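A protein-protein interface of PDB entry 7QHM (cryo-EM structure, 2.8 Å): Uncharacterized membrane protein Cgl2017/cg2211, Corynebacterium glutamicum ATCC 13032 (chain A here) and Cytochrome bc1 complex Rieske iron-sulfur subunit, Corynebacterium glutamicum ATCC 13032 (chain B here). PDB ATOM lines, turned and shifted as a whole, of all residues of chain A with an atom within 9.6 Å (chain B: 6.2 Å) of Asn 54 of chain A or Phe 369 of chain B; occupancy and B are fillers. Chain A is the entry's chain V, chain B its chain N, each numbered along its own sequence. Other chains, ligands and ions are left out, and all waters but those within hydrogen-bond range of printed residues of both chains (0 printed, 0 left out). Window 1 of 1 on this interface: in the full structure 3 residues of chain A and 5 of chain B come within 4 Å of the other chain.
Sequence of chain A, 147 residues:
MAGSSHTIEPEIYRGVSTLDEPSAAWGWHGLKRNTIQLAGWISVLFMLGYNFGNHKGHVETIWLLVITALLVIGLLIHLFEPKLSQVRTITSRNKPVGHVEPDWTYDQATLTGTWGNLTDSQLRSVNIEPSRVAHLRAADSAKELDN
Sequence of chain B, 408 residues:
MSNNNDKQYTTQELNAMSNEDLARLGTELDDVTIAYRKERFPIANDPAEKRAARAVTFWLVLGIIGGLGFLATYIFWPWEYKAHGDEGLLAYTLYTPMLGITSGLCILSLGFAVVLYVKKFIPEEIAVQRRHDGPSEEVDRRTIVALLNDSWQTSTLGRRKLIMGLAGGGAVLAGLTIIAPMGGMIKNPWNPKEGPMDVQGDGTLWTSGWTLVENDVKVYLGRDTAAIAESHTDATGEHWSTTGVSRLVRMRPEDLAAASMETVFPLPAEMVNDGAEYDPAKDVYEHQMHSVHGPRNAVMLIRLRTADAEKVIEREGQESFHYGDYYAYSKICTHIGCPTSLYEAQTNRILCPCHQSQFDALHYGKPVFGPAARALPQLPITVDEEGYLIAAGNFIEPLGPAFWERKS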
ATOM      1  N   GLY A  49     -23.426 -15.892  15.528  1.00  0.00           N
ATOM      2  CA  GLY A  49     -23.617 -16.838  16.612  1.00  0.00           C
ATOM      3  C   GLY A  49     -22.575 -16.726  17.706  1.00  0.00           C
ATOM      4  O   GLY A  49     -22.858 -17.030  18.868  1.00  0.00           O
ATOM      5  N   TYR A  50     -21.370 -16.270  17.364  1.00  0.00           N
ATOM      6  CA  TYR A  50     -20.342 -16.098  18.380  1.00  0.00           C
ATOM      7  C   TYR A  50     -20.733 -15.075  19.436  1.00  0.00           C
ATOM      8  O   TYR A  50     -20.224 -15.136  20.556  1.00  0.00           O
ATOM      9  CB  TYR A  50     -19.026 -15.658  17.748  1.00  0.00           C
ATOM     10  CG  TYR A  50     -18.293 -16.677  16.905  1.00  0.00           C
ATOM     11  CD1 TYR A  50     -18.329 -18.026  17.200  1.00  0.00           C
ATOM     12  CD2 TYR A  50     -17.530 -16.268  15.826  1.00  0.00           C
ATOM     13  CE1 TYR A  50     -17.654 -18.932  16.437  1.00  0.00           C
ATOM     14  CE2 TYR A  50     -16.854 -17.166  15.060  1.00  0.00           C
ATOM     15  CZ  TYR A  50     -16.919 -18.499  15.367  1.00  0.00           C
ATOM     16  OH  TYR A  50     -16.230 -19.395  14.596  1.00  0.00           O
ATOM     17  N   ASN A  51     -21.622 -14.137  19.112  1.00  0.00           N
ATOM     18  CA  ASN A  51     -22.072 -13.180  20.112  1.00  0.00           C
ATOM     19  C   ASN A  51     -22.814 -13.847  21.251  1.00  0.00           C
ATOM     20  O   ASN A  51     -22.954 -13.236  22.312  1.00  0.00           O
ATOM     21  CB  ASN A  51     -22.990 -12.129  19.497  1.00  0.00           C
ATOM     22  CG  ASN A  51     -22.293 -11.257  18.503  1.00  0.00           C
ATOM     23  OD1 ASN A  51     -21.673 -10.262  18.860  1.00  0.00           O
ATOM     24  ND2 ASN A  51     -22.407 -11.610  17.239  1.00  0.00           N
ATOM     25  N   PHE A  52     -23.318 -15.063  21.052  1.00  0.00           N
ATOM     26  CA  PHE A  52     -23.978 -15.813  22.114  1.00  0.00           C
ATOM     27  C   PHE A  52     -22.930 -16.730  22.731  1.00  0.00           C
ATOM     28  O   PHE A  52     -22.702 -17.846  22.272  1.00  0.00           O
ATOM     29  CB  PHE A  52     -25.186 -16.558  21.566  1.00  0.00           C
ATOM     30  CG  PHE A  52     -26.134 -15.666  20.831  1.00  0.00           C
ATOM     31  CD1 PHE A  52     -26.991 -14.836  21.512  1.00  0.00           C
ATOM     32  CD2 PHE A  52     -26.141 -15.630  19.456  1.00  0.00           C
ATOM     33  CE1 PHE A  52     -27.843 -14.003  20.834  1.00  0.00           C
ATOM     34  CE2 PHE A  52     -26.998 -14.795  18.777  1.00  0.00           C
ATOM     35  CZ  PHE A  52     -27.844 -13.982  19.469  1.00  0.00           C
ATOM     36  N   GLY A  53     -22.270 -16.229  23.771  1.00  0.00           N
ATOM     37  CA  GLY A  53     -21.235 -16.962  24.472  1.00  0.00           C
ATOM     38  C   GLY A  53     -21.102 -16.417  25.875  1.00  0.00           C
ATOM     39  O   GLY A  53     -21.743 -15.429  26.240  1.00  0.00           O
ATOM     40  N   ASN A  54     -20.249 -17.065  26.668  1.00  0.00           N
ATOM     41  CA  ASN A  54     -20.099 -16.704  28.072  1.00  0.00           C
ATOM     42  C   ASN A  54     -19.072 -15.599  28.307  1.00  0.00           C
ATOM     43  O   ASN A  54     -18.666 -15.387  29.451  1.00  0.00           O
ATOM     44  CB  ASN A  54     -19.754 -17.938  28.911  1.00  0.00           C
ATOM     45  CG  ASN A  54     -18.470 -18.608  28.500  1.00  0.00           C
ATOM     46  OD1 ASN A  54     -17.678 -18.066  27.740  1.00  0.00           O
ATOM     47  ND2 ASN A  54     -18.257 -19.805  29.011  1.00  0.00           N
ATOM     48  N   HIS A  55     -18.671 -14.878  27.269  1.00  0.00           N
ATOM     49  CA  HIS A  55     -17.628 -13.867  27.405  1.00  0.00           C
ATOM     50  C   HIS A  55     -18.208 -12.544  27.885  1.00  0.00           C
ATOM     51  O   HIS A  55     -19.378 -12.233  27.661  1.00  0.00           O
ATOM     52  CB  HIS A  55     -16.879 -13.661  26.086  1.00  0.00           C
ATOM     53  CG  HIS A  55     -17.765 -13.378  24.913  1.00  0.00           C
ATOM     54  ND1 HIS A  55     -18.178 -12.110  24.578  1.00  0.00           N
ATOM     55  CD2 HIS A  55     -18.321 -14.209  24.003  1.00  0.00           C
ATOM     56  CE1 HIS A  55     -18.952 -12.172  23.512  1.00  0.00           C
ATOM     57  NE2 HIS A  55     -19.054 -13.435  23.144  1.00  0.00           N
ATOM     58  N   LYS A  56     -17.358 -11.756  28.545  1.00  0.00           N
ATOM     59  CA  LYS A  56     -17.783 -10.570  29.274  1.00  0.00           C
ATOM     60  C   LYS A  56     -17.405  -9.256  28.612  1.00  0.00           C
ATOM     61  O   LYS A  56     -18.066  -8.250  28.869  1.00  0.00           O
ATOM     62  CB  LYS A  56     -17.189 -10.579  30.691  1.00  0.00           C
ATOM     63  CG  LYS A  56     -17.646 -11.732  31.596  1.00  0.00           C
ATOM     64  CD  LYS A  56     -19.169 -11.817  31.788  1.00  0.00           C
ATOM     65  CE  LYS A  56     -19.779 -10.566  32.421  1.00  0.00           C
ATOM     66  NZ  LYS A  56     -19.291 -10.334  33.808  1.00  0.00           N
ATOM     67  N   GLY A  57     -16.369  -9.236  27.785  1.00  0.00           N
ATOM     68  CA  GLY A  57     -15.926  -8.009  27.159  1.00  0.00           C
ATOM     69  C   GLY A  57     -16.566  -7.806  25.801  1.00  0.00           C
ATOM     70  O   GLY A  57     -16.900  -8.758  25.105  1.00  0.00           O
ATOM     71  N   HIS A  58     -16.707  -6.539  25.419  1.00  0.00           N
ATOM     72  CA  HIS A  58     -17.345  -6.158  24.170  1.00  0.00           C
ATOM     73  C   HIS A  58     -16.367  -5.614  23.143  1.00  0.00           C
ATOM     74  O   HIS A  58     -16.797  -5.141  22.089  1.00  0.00           O
ATOM     75  CB  HIS A  58     -18.446  -5.143  24.447  1.00  0.00           C
ATOM     76  CG  HIS A  58     -19.598  -5.718  25.203  1.00  0.00           C
ATOM     77  ND1 HIS A  58     -19.879  -5.377  26.506  1.00  0.00           N
ATOM     78  CD2 HIS A  58     -20.523  -6.637  24.845  1.00  0.00           C
ATOM     79  CE1 HIS A  58     -20.936  -6.054  26.915  1.00  0.00           C
ATOM     80  NE2 HIS A  58     -21.346  -6.825  25.925  1.00  0.00           N
ATOM     81  N   GLU A  60     -14.539  -7.786  21.801  1.00  0.00           N
ATOM     82  CA  GLU A  60     -14.869  -8.922  20.957  1.00  0.00           C
ATOM     83  C   GLU A  60     -16.089  -8.620  20.106  1.00  0.00           C
ATOM     84  O   GLU A  60     -16.129  -8.942  18.914  1.00  0.00           O
ATOM     85  CB  GLU A  60     -15.150 -10.136  21.837  1.00  0.00           C
ATOM     86  CG  GLU A  60     -14.009 -10.682  22.692  1.00  0.00           C
ATOM     87  CD  GLU A  60     -13.613  -9.853  23.903  1.00  0.00           C
ATOM     88  OE1 GLU A  60     -14.344  -8.912  24.248  1.00  0.00           O
ATOM     89  OE2 GLU A  60     -12.566 -10.151  24.515  1.00  0.00           O
ATOM     90  N   HIS B 355      -8.123 -25.789  27.824  1.00  0.00           N
ATOM     91  CA  HIS B 355      -8.780 -24.988  26.796  1.00  0.00           C
ATOM     92  C   HIS B 355      -9.206 -23.624  27.312  1.00  0.00           C
ATOM     93  O   HIS B 355     -10.167 -23.045  26.804  1.00  0.00           O
ATOM     94  CB  HIS B 355      -9.987 -25.714  26.211  1.00  0.00           C
ATOM     95  CG  HIS B 355      -9.760 -27.171  25.999  1.00  0.00           C
ATOM     96  ND1 HIS B 355     -10.224 -28.126  26.873  1.00  0.00           N
ATOM     97  CD2 HIS B 355      -9.103 -27.836  25.024  1.00  0.00           C
ATOM     98  CE1 HIS B 355      -9.854 -29.318  26.446  1.00  0.00           C
ATOM     99  NE2 HIS B 355      -9.180 -29.171  25.321  1.00  0.00           N
ATOM    100  N   GLN B 356      -8.499 -23.092  28.306  1.00  0.00           N
ATOM    101  CA  GLN B 356      -8.580 -21.675  28.666  1.00  0.00           C
ATOM    102  C   GLN B 356      -9.982 -21.255  29.094  1.00  0.00           C
ATOM    103  O   GLN B 356     -10.461 -20.181  28.732  1.00  0.00           O
ATOM    104  CB  GLN B 356      -8.096 -20.787  27.519  1.00  0.00           C
ATOM    105  CG  GLN B 356      -6.626 -20.881  27.240  1.00  0.00           C
ATOM    106  CD  GLN B 356      -6.235 -22.078  26.435  1.00  0.00           C
ATOM    107  OE1 GLN B 356      -5.429 -22.891  26.874  1.00  0.00           O
ATOM    108  NE2 GLN B 356      -6.775 -22.186  25.237  1.00  0.00           N
ATOM    109  N   SER B 357     -10.646 -22.089  29.880  1.00  0.00           N
ATOM    110  CA  SER B 357     -11.866 -21.659  30.540  1.00  0.00           C
ATOM    111  C   SER B 357     -11.509 -20.849  31.770  1.00  0.00           C
ATOM    112  O   SER B 357     -10.559 -21.170  32.484  1.00  0.00           O
ATOM    113  CB  SER B 357     -12.728 -22.848  30.930  1.00  0.00           C
ATOM    114  OG  SER B 357     -13.277 -23.470  29.794  1.00  0.00           O
ATOM    115  N   GLN B 358     -12.272 -19.791  32.009  1.00  0.00           N
ATOM    116  CA  GLN B 358     -12.057 -18.890  33.127  1.00  0.00           C
ATOM    117  C   GLN B 358     -13.324 -18.823  33.952  1.00  0.00           C
ATOM    118  O   GLN B 358     -14.407 -18.602  33.409  1.00  0.00           O
ATOM    119  CB  GLN B 358     -11.664 -17.506  32.639  1.00  0.00           C
ATOM    120  CG  GLN B 358     -10.273 -17.473  32.090  1.00  0.00           C
ATOM    121  CD  GLN B 358     -10.102 -16.445  31.026  1.00  0.00           C
ATOM    122  OE1 GLN B 358     -10.429 -15.281  31.219  1.00  0.00           O
ATOM    123  NE2 GLN B 358      -9.599 -16.865  29.879  1.00  0.00           N
ATOM    124  N   PHE B 359     -13.183 -19.026  35.255  1.00  0.00           N
ATOM    125  CA  PHE B 359     -14.289 -19.027  36.195  1.00  0.00           C
ATOM    126  C   PHE B 359     -14.088 -17.894  37.182  1.00  0.00           C
ATOM    127  O   PHE B 359     -12.986 -17.703  37.693  1.00  0.00           O
ATOM    128  CB  PHE B 359     -14.371 -20.348  36.949  1.00  0.00           C
ATOM    129  CG  PHE B 359     -14.380 -21.557  36.065  1.00  0.00           C
ATOM    130  CD1 PHE B 359     -13.205 -22.170  35.700  1.00  0.00           C
ATOM    131  CD2 PHE B 359     -15.564 -22.092  35.615  1.00  0.00           C
ATOM    132  CE1 PHE B 359     -13.217 -23.272  34.901  1.00  0.00           C
ATOM    133  CE2 PHE B 359     -15.567 -23.196  34.821  1.00  0.00           C
ATOM    134  CZ  PHE B 359     -14.398 -23.784  34.467  1.00  0.00           C
ATOM    135  N   PRO B 367     -18.496 -19.532  34.696  1.00  0.00           N
ATOM    136  CA  PRO B 367     -17.550 -19.259  33.612  1.00  0.00           C
ATOM    137  C   PRO B 367     -17.711 -17.871  33.022  1.00  0.00           C
ATOM    138  O   PRO B 367     -18.814 -17.332  32.926  1.00  0.00           O
ATOM    139  CB  PRO B 367     -17.883 -20.333  32.576  1.00  0.00           C
ATOM    140  CG  PRO B 367     -18.514 -21.382  33.316  1.00  0.00           C
ATOM    141  CD  PRO B 367     -19.298 -20.722  34.376  1.00  0.00           C
ATOM    142  N   VAL B 368     -16.578 -17.300  32.613  1.00  0.00           N
ATOM    143  CA  VAL B 368     -16.530 -16.005  31.949  1.00  0.00           C
ATOM    144  C   VAL B 368     -15.754 -16.048  30.644  1.00  0.00           C
ATOM    145  O   VAL B 368     -15.563 -15.008  30.018  1.00  0.00           O
ATOM    146  CB  VAL B 368     -15.941 -14.922  32.881  1.00  0.00           C
ATOM    147  CG1 VAL B 368     -16.818 -14.742  34.092  1.00  0.00           C
ATOM    148  CG2 VAL B 368     -14.514 -15.256  33.308  1.00  0.00           C
ATOM    149  N   PHE B 369     -15.281 -17.213  30.222  1.00  0.00           N
ATOM    150  CA  PHE B 369     -14.506 -17.355  29.002  1.00  0.00           C
ATOM    151  C   PHE B 369     -14.303 -18.840  28.758  1.00  0.00           C
ATOM    152  O   PHE B 369     -14.394 -19.649  29.682  1.00  0.00           O
ATOM    153  CB  PHE B 369     -13.157 -16.641  29.094  1.00  0.00           C
ATOM    154  CG  PHE B 369     -12.581 -16.295  27.775  1.00  0.00           C
ATOM    155  CD1 PHE B 369     -12.928 -15.125  27.151  1.00  0.00           C
ATOM    156  CD2 PHE B 369     -11.695 -17.140  27.153  1.00  0.00           C
ATOM    157  CE1 PHE B 369     -12.406 -14.806  25.939  1.00  0.00           C
ATOM    158  CE2 PHE B 369     -11.167 -16.825  25.939  1.00  0.00           C
ATOM    159  CZ  PHE B 369     -11.521 -15.658  25.331  1.00  0.00           C
ATOM    160  N   GLY B 370     -14.049 -19.191  27.505  1.00  0.00           N
ATOM    161  CA  GLY B 370     -13.736 -20.551  27.141  1.00  0.00           C
ATOM    162  C   GLY B 370     -14.970 -21.382  26.894  1.00  0.00           C
ATOM    163  O   GLY B 370     -16.089 -20.874  26.858  1.00  0.00           O
ATOM    164  N   PRO B 371     -14.794 -22.690  26.722  1.00  0.00           N
ATOM    165  CA  PRO B 371     -15.924 -23.559  26.381  1.00  0.00           C
ATOM    166  C   PRO B 371     -16.707 -24.135  27.547  1.00  0.00           C
ATOM    167  O   PRO B 371     -17.688 -24.840  27.300  1.00  0.00           O
ATOM    168  CB  PRO B 371     -15.240 -24.677  25.598  1.00  0.00           C
ATOM    169  CG  PRO B 371     -13.898 -24.752  26.166  1.00  0.00           C
ATOM    170  CD  PRO B 371     -13.505 -23.362  26.504  1.00  0.00           C
ATOM    171  N   ALA B 372     -16.332 -23.875  28.792  1.00  0.00           N
ATOM    172  CA  ALA B 372     -17.128 -24.359  29.909  1.00  0.00           C
ATOM    173  C   ALA B 372     -18.435 -23.582  30.003  1.00  0.00           C
ATOM    174  O   ALA B 372     -18.496 -22.391  29.696  1.00  0.00           O
ATOM    175  CB  ALA B 372     -16.348 -24.237  31.212  1.00  0.00           C
ATOM    176  N   ALA B 373     -19.490 -24.278  30.420  1.00  0.00           N
ATOM    177  CA  ALA B 373     -20.828 -23.713  30.531  1.00  0.00           C
ATOM    178  C   ALA B 373     -21.387 -23.743  31.938  1.00  0.00           C
ATOM    179  O   ALA B 373     -22.228 -22.911  32.270  1.00  0.00           O
ATOM    180  CB  ALA B 373     -21.798 -24.464  29.612  1.00  0.00           C
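O of Gly 370 of chain B lies within hydrogen-bond range of ND2 of Asn 54 of chain A (3.2 Å).
The backbone carbonyl oxygen of Ala 372 of chain B lies within hydrogen-bond range of the side-chain amide nitrogen of Asn 54 of chain A (2.7 Å).
O of Val 368 of chain B sits close to O of Asn 54 of chain A, at 3.2 Å.
OG of Ser 357 of chain B lies within hydrogen-bond range of N of Ala 372 of chain B, 3.2 Å away.
The backbone carbonyl oxygen of Gln 358 of chain B sits at hydrogen-bond distance from the backbone NH of Val 368 of chain B (2.7 Å).
O of Phe 369 of chain B is in hydrogen-bond range of N of Gln 358 of chain B (3.2 Å).
The backbone carbonyl oxygen (O) of Tyr 50 of chain A is in hydrogen-bond range of a ring nitrogen (NE2) of His 55 of chain A (3.3 Å).
Among the printed residues, merely in contact across the chains: Asn 54 of chain A with Phe 369 of chain B (3.5 Å), His 55 of chain A with Val 368 of chain B (3.5 Å), Asn 54 of chain A with Pro 367 of chain B (3.6 Å) and Lys 56 of chain A with Val 368 of chain B (3.8 Å).
Printed residues of chain B within 4 Å of Asn 54 of chain A: Pro 367, Val 368, Phe 369, Gly 370 and Ala 372.
Of chain A, only Asn 54 (3.5 Å) comes within 4 Å of Phe 369 of chain B.
No residue of chain A comes within 4 Å of Gln 358 of chain B.
Gly 370 of chain B touches one residue of chain A.
Of the printed residues of chain A, Pro 367 of chain B touches Asn 54 (3.6 Å).
Of the printed residues of chain B, His 55 of chain A touches Val 368 (3.5 Å).
Ala 373 of chain B touches none of the printed residues of chain A.
Pro 371 of chain B touches none of the printed residues of chain A.
Of the 12 printed residues of chain B, 5 touch a printed residue of chain A.
Hydrophobic or aromatic side chains of chain B within 4 Å of the printed part of chain A: Pro 367 and Val 368.
Of the 11 printed residues of chain A, 3 touch a printed residue of chain B.
Among the printed residues, 7 pairs touch across the chains.
Among the printed residues, no Asp or Glu carboxylate lies within 4 Å of a Lys or Arg side-chain nitrogen of the other chain.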
